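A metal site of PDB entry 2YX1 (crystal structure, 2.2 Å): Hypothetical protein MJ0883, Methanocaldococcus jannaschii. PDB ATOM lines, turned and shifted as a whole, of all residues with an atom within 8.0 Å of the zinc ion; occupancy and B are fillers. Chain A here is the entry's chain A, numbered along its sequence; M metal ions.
The backbone NH of Asp 308 lies within hydrogen-bond range of the backbone carbonyl oxygen of Lys 335 (3.1 Å).
The backbone carbonyl oxygen (O) of Asp 308 lies within hydrogen-bond range of the backbone NH (N) of Asn 334 (2.9 Å).
N of Glu 304 touches the zinc ion, at 3.7 Å.
Asp 308 touches the zinc ion.
Of the 20 residues printed, 5 come within 4 Å of the zinc ion.
The nearest printed residue that does not touch the zinc ion is Lys 306 (4.4 Å).
The zinc ion is bound by O of Phe 303 (2.2 Å), SG of Cys 307 (2.4 Å) and SG of Cys 309 (2.5 Å).
Slightly farther from the zinc ion lies the backbone carbonyl oxygen (O) of Cys 307 (2.6 Å).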
ATOM      1  N   ILE A 274     -11.124  16.030  -8.101  1.00  0.00           N
ATOM      2  CA  ILE A 274     -11.653  14.782  -8.646  1.00  0.00           C
ATOM      3  C   ILE A 274     -10.851  14.219  -9.812  1.00  0.00           C
ATOM      4  O   ILE A 274     -10.671  13.012  -9.900  1.00  0.00           O
ATOM      5  CB  ILE A 274     -13.129  14.926  -9.090  1.00  0.00           C
ATOM      6  CG1 ILE A 274     -13.951  15.524  -7.956  1.00  0.00           C
ATOM      7  CG2 ILE A 274     -13.705  13.569  -9.507  1.00  0.00           C
ATOM      8  CD1 ILE A 274     -15.431  15.730  -8.290  1.00  0.00           C
ATOM      9  N   LEU A 278      -9.298  10.475  -9.808  1.00  0.00           N
ATOM     10  CA  LEU A 278      -9.591   9.441 -10.815  1.00  0.00           C
ATOM     11  C   LEU A 278      -8.305   8.937 -11.466  1.00  0.00           C
ATOM     12  O   LEU A 278      -8.251   7.817 -11.973  1.00  0.00           O
ATOM     13  CB  LEU A 278     -10.551   9.980 -11.882  1.00  0.00           C
ATOM     14  CG  LEU A 278     -11.989  10.279 -11.399  1.00  0.00           C
ATOM     15  CD1 LEU A 278     -12.737  11.061 -12.451  1.00  0.00           C
ATOM     16  CD2 LEU A 278     -12.719   8.987 -11.082  1.00  0.00           C
ATOM     17  N   ALA A 299     -22.912  16.221  -6.052  1.00  0.00           N
ATOM     18  CA  ALA A 299     -21.740  15.335  -6.030  1.00  0.00           C
ATOM     19  C   ALA A 299     -21.915  14.162  -6.974  1.00  0.00           C
ATOM     20  O   ALA A 299     -21.001  13.789  -7.709  1.00  0.00           O
ATOM     21  CB  ALA A 299     -21.489  14.847  -4.594  1.00  0.00           C
ATOM     22  N   ILE A 300     -23.099  13.564  -6.955  1.00  0.00           N
ATOM     23  CA  ILE A 300     -23.388  12.439  -7.834  1.00  0.00           C
ATOM     24  C   ILE A 300     -23.226  12.869  -9.291  1.00  0.00           C
ATOM     25  O   ILE A 300     -22.570  12.187 -10.090  1.00  0.00           O
ATOM     26  CB  ILE A 300     -24.820  11.916  -7.584  1.00  0.00           C
ATOM     27  CG1 ILE A 300     -24.882  11.264  -6.197  1.00  0.00           C
ATOM     28  CG2 ILE A 300     -25.227  10.899  -8.695  1.00  0.00           C
ATOM     29  CD1 ILE A 300     -26.214  10.666  -5.859  1.00  0.00           C
ATOM     30  N   LYS A 301     -23.799  14.009  -9.636  1.00  0.00           N
ATOM     31  CA  LYS A 301     -23.696  14.516 -10.997  1.00  0.00           C
ATOM     32  C   LYS A 301     -22.247  14.772 -11.420  1.00  0.00           C
ATOM     33  O   LYS A 301     -21.859  14.429 -12.539  1.00  0.00           O
ATOM     34  CB  LYS A 301     -24.505  15.803 -11.134  1.00  0.00           C
ATOM     35  CG  LYS A 301     -24.508  16.394 -12.520  1.00  0.00           C
ATOM     36  CD  LYS A 301     -25.365  17.646 -12.537  1.00  0.00           C
ATOM     37  CE  LYS A 301     -25.381  18.279 -13.911  1.00  0.00           C
ATOM     38  NZ  LYS A 301     -25.971  19.657 -13.868  1.00  0.00           N
ATOM     39  N   LEU A 302     -21.441  15.382 -10.550  1.00  0.00           N
ATOM     40  CA  LEU A 302     -20.038  15.659 -10.885  1.00  0.00           C
ATOM     41  C   LEU A 302     -19.337  14.351 -11.232  1.00  0.00           C
ATOM     42  O   LEU A 302     -18.659  14.269 -12.245  1.00  0.00           O
ATOM     43  CB  LEU A 302     -19.319  16.333  -9.708  1.00  0.00           C
ATOM     44  CG  LEU A 302     -18.492  17.580 -10.063  1.00  0.00           C
ATOM     45  CD1 LEU A 302     -18.121  18.316  -8.777  1.00  0.00           C
ATOM     46  CD2 LEU A 302     -17.254  17.185 -10.843  1.00  0.00           C
ATOM     47  N   PHE A 303     -19.542  13.322 -10.407  1.00  0.00           N
ATOM     48  CA  PHE A 303     -18.926  12.017 -10.661  1.00  0.00           C
ATOM     49  C   PHE A 303     -19.513  11.307 -11.867  1.00  0.00           C
ATOM     50  O   PHE A 303     -18.771  10.708 -12.644  1.00  0.00           O
ATOM     51  CB  PHE A 303     -19.017  11.104  -9.422  1.00  0.00           C
ATOM     52  CG  PHE A 303     -17.873  11.286  -8.443  1.00  0.00           C
ATOM     53  CD1 PHE A 303     -17.834  12.383  -7.576  1.00  0.00           C
ATOM     54  CD2 PHE A 303     -16.810  10.383  -8.431  1.00  0.00           C
ATOM     55  CE1 PHE A 303     -16.739  12.601  -6.720  1.00  0.00           C
ATOM     56  CE2 PHE A 303     -15.706  10.591  -7.579  1.00  0.00           C
ATOM     57  CZ  PHE A 303     -15.678  11.714  -6.726  1.00  0.00           C
ATOM     58  N   GLU A 304     -20.828  11.354 -12.056  1.00  0.00           N
ATOM     59  CA  GLU A 304     -21.413  10.685 -13.209  1.00  0.00           C
ATOM     60  C   GLU A 304     -20.887  11.212 -14.537  1.00  0.00           C
ATOM     61  O   GLU A 304     -20.707  10.449 -15.489  1.00  0.00           O
ATOM     62  CB  GLU A 304     -22.925  10.768 -13.201  1.00  0.00           C
ATOM     63  CG  GLU A 304     -23.539   9.838 -12.178  1.00  0.00           C
ATOM     64  CD  GLU A 304     -25.042   9.765 -12.310  1.00  0.00           C
ATOM     65  OE1 GLU A 304     -25.664  10.811 -12.591  1.00  0.00           O
ATOM     66  OE2 GLU A 304     -25.595   8.649 -12.110  1.00  0.00           O
ATOM     67  N   LYS A 305     -20.603  12.510 -14.588  1.00  0.00           N
ATOM     68  CA  LYS A 305     -20.097  13.088 -15.819  1.00  0.00           C
ATOM     69  C   LYS A 305     -18.609  12.796 -16.037  1.00  0.00           C
ATOM     70  O   LYS A 305     -18.144  12.748 -17.175  1.00  0.00           O
ATOM     71  CB  LYS A 305     -20.341  14.608 -15.819  1.00  0.00           C
ATOM     72  CG  LYS A 305     -19.200  15.473 -15.334  1.00  0.00           C
ATOM     73  CD  LYS A 305     -19.548  16.943 -15.522  1.00  0.00           C
ATOM     74  CE  LYS A 305     -18.455  17.886 -15.017  1.00  0.00           C
ATOM     75  NZ  LYS A 305     -17.192  17.769 -15.793  1.00  0.00           N
ATOM     76  N   LYS A 306     -17.879  12.571 -14.949  1.00  0.00           N
ATOM     77  CA  LYS A 306     -16.445  12.294 -15.057  1.00  0.00           C
ATOM     78  C   LYS A 306     -16.079  10.831 -15.307  1.00  0.00           C
ATOM     79  O   LYS A 306     -14.988  10.549 -15.786  1.00  0.00           O
ATOM     80  CB  LYS A 306     -15.722  12.789 -13.809  1.00  0.00           C
ATOM     81  CG  LYS A 306     -15.920  14.265 -13.481  1.00  0.00           C
ATOM     82  CD  LYS A 306     -14.695  15.064 -13.812  1.00  0.00           C
ATOM     83  CE  LYS A 306     -14.779  16.449 -13.203  1.00  0.00           C
ATOM     84  NZ  LYS A 306     -13.555  17.235 -13.530  1.00  0.00           N
ATOM     85  N   CYS A 307     -16.973   9.901 -15.008  1.00  0.00           N
ATOM     86  CA  CYS A 307     -16.633   8.509 -15.215  1.00  0.00           C
ATOM     87  C   CYS A 307     -17.874   7.654 -14.982  1.00  0.00           C
ATOM     88  O   CYS A 307     -18.927   8.171 -14.636  1.00  0.00           O
ATOM     89  CB  CYS A 307     -15.521   8.099 -14.234  1.00  0.00           C
ATOM     90  SG  CYS A 307     -15.937   8.230 -12.408  1.00  0.00           S
ATOM     91  N   ASP A 308     -17.749   6.358 -15.225  1.00  0.00           N
ATOM     92  CA  ASP A 308     -18.865   5.444 -14.980  1.00  0.00           C
ATOM     93  C   ASP A 308     -18.676   4.920 -13.552  1.00  0.00           C
ATOM     94  O   ASP A 308     -17.727   4.197 -13.255  1.00  0.00           O
ATOM     95  CB  ASP A 308     -18.841   4.278 -15.979  1.00  0.00           C
ATOM     96  CG  ASP A 308     -19.792   3.162 -15.583  1.00  0.00           C
ATOM     97  OD1 ASP A 308     -20.902   3.464 -15.073  1.00  0.00           O
ATOM     98  OD2 ASP A 308     -19.438   1.974 -15.786  1.00  0.00           O
ATOM     99  N   CYS A 309     -19.610   5.285 -12.674  1.00  0.00           N
ATOM    100  CA  CYS A 309     -19.507   4.896 -11.273  1.00  0.00           C
ATOM    101  C   CYS A 309     -20.826   4.605 -10.574  1.00  0.00           C
ATOM    102  O   CYS A 309     -21.908   4.944 -11.053  1.00  0.00           O
ATOM    103  CB  CYS A 309     -18.802   6.017 -10.513  1.00  0.00           C
ATOM    104  SG  CYS A 309     -19.790   7.539 -10.524  1.00  0.00           S
ATOM    105  N   GLU A 310     -20.721   3.994  -9.414  1.00  0.00           N
ATOM    106  CA  GLU A 310     -21.891   3.663  -8.623  1.00  0.00           C
ATOM    107  C   GLU A 310     -21.669   4.078  -7.174  1.00  0.00           C
ATOM    108  O   GLU A 310     -20.574   3.915  -6.623  1.00  0.00           O
ATOM    109  CB  GLU A 310     -22.157   2.156  -8.710  1.00  0.00           C
ATOM    110  CG  GLU A 310     -23.247   1.654  -7.766  1.00  0.00           C
ATOM    111  CD  GLU A 310     -23.237   0.133  -7.635  1.00  0.00           C
ATOM    112  OE1 GLU A 310     -22.379  -0.500  -8.290  1.00  0.00           O
ATOM    113  OE2 GLU A 310     -24.083  -0.408  -6.871  1.00  0.00           O
ATOM    114  N   PHE A 331     -17.924   6.094  -3.859  1.00  0.00           N
ATOM    115  CA  PHE A 331     -18.179   5.846  -5.271  1.00  0.00           C
ATOM    116  C   PHE A 331     -17.345   4.701  -5.803  1.00  0.00           C
ATOM    117  O   PHE A 331     -16.133   4.732  -5.692  1.00  0.00           O
ATOM    118  CB  PHE A 331     -17.824   7.079  -6.098  1.00  0.00           C
ATOM    119  CG  PHE A 331     -18.725   8.249  -5.871  1.00  0.00           C
ATOM    120  CD1 PHE A 331     -19.957   8.322  -6.517  1.00  0.00           C
ATOM    121  CD2 PHE A 331     -18.314   9.302  -5.079  1.00  0.00           C
ATOM    122  CE1 PHE A 331     -20.769   9.455  -6.391  1.00  0.00           C
ATOM    123  CE2 PHE A 331     -19.116  10.439  -4.940  1.00  0.00           C
ATOM    124  CZ  PHE A 331     -20.350  10.515  -5.598  1.00  0.00           C
ATOM    125  N   LYS A 332     -17.973   3.703  -6.390  1.00  0.00           N
ATOM    126  CA  LYS A 332     -17.191   2.642  -6.996  1.00  0.00           C
ATOM    127  C   LYS A 332     -16.938   3.121  -8.438  1.00  0.00           C
ATOM    128  O   LYS A 332     -17.875   3.509  -9.144  1.00  0.00           O
ATOM    129  CB  LYS A 332     -17.929   1.313  -6.995  1.00  0.00           C
ATOM    130  CG  LYS A 332     -17.068   0.198  -7.563  1.00  0.00           C
ATOM    131  CD  LYS A 332     -17.829  -1.079  -7.739  1.00  0.00           C
ATOM    132  CE  LYS A 332     -16.887  -2.191  -8.131  1.00  0.00           C
ATOM    133  NZ  LYS A 332     -17.651  -3.422  -8.496  1.00  0.00           N
ATOM    134  N   ILE A 333     -15.674   3.123  -8.841  1.00  0.00           N
ATOM    135  CA  ILE A 333     -15.244   3.576 -10.165  1.00  0.00           C
ATOM    136  C   ILE A 333     -15.124   2.368 -11.112  1.00  0.00           C
ATOM    137  O   ILE A 333     -14.120   1.644 -11.100  1.00  0.00           O
ATOM    138  CB  ILE A 333     -13.883   4.322 -10.063  1.00  0.00           C
ATOM    139  CG1 ILE A 333     -13.883   5.289  -8.853  1.00  0.00           C
ATOM    140  CG2 ILE A 333     -13.597   5.073 -11.350  1.00  0.00           C
ATOM    141  CD1 ILE A 333     -15.011   6.347  -8.847  1.00  0.00           C
ATOM    142  N   ASN A 334     -16.141   2.171 -11.936  1.00  0.00           N
ATOM    143  CA  ASN A 334     -16.173   1.035 -12.865  1.00  0.00           C
ATOM    144  C   ASN A 334     -15.266   1.205 -14.087  1.00  0.00           C
ATOM    145  O   ASN A 334     -14.530   0.281 -14.446  1.00  0.00           O
ATOM    146  CB  ASN A 334     -17.632   0.755 -13.229  1.00  0.00           C
ATOM    147  CG  ASN A 334     -18.401   0.252 -12.021  1.00  0.00           C
ATOM    148  OD1 ASN A 334     -19.546   0.617 -11.785  1.00  0.00           O
ATOM    149  ND2 ASN A 334     -17.759  -0.623 -11.255  1.00  0.00           N
ATOM    150  N   LYS A 335     -15.329   2.357 -14.738  1.00  0.00           N
ATOM    151  CA  LYS A 335     -14.411   2.602 -15.849  1.00  0.00           C
ATOM    152  C   LYS A 335     -14.138   4.087 -15.909  1.00  0.00           C
ATOM    153  O   LYS A 335     -15.019   4.901 -15.639  1.00  0.00           O
ATOM    154  CB  LYS A 335     -14.974   2.096 -17.193  1.00  0.00           C
ATOM    155  CG  LYS A 335     -16.047   2.948 -17.835  1.00  0.00           C
ATOM    156  CD  LYS A 335     -15.956   2.871 -19.357  1.00  0.00           C
ATOM    157  CE  LYS A 335     -15.986   1.432 -19.850  1.00  0.00           C
ATOM    158  NZ  LYS A 335     -15.697   1.335 -21.316  1.00  0.00           N
ATOM    159  N   LYS A 336     -12.902   4.452 -16.248  1.00  0.00           N
ATOM    160  CA  LYS A 336     -12.541   5.859 -16.313  1.00  0.00           C
ATOM    161  C   LYS A 336     -12.620   6.456 -17.719  1.00  0.00           C
ATOM    162  O   LYS A 336     -12.978   5.708 -18.656  1.00  0.00           O
ATOM    163  CB  LYS A 336     -11.124   6.040 -15.734  1.00  0.00           C
ATOM    164  CG  LYS A 336     -11.030   5.500 -14.311  1.00  0.00           C
ATOM    165  CD  LYS A 336      -9.744   5.906 -13.618  1.00  0.00           C
ATOM    166  CE  LYS A 336      -8.553   5.156 -14.139  1.00  0.00           C
ATOM    167  NZ  LYS A 336      -7.331   5.515 -13.383  1.00  0.00           N
ATOM    168  OXT LYS A 336     -12.341   7.672 -17.875  1.00  0.00           O
HETATM  169 ZN    ZN M   1     -18.288   8.661 -12.160  1.00  0.00          ZN
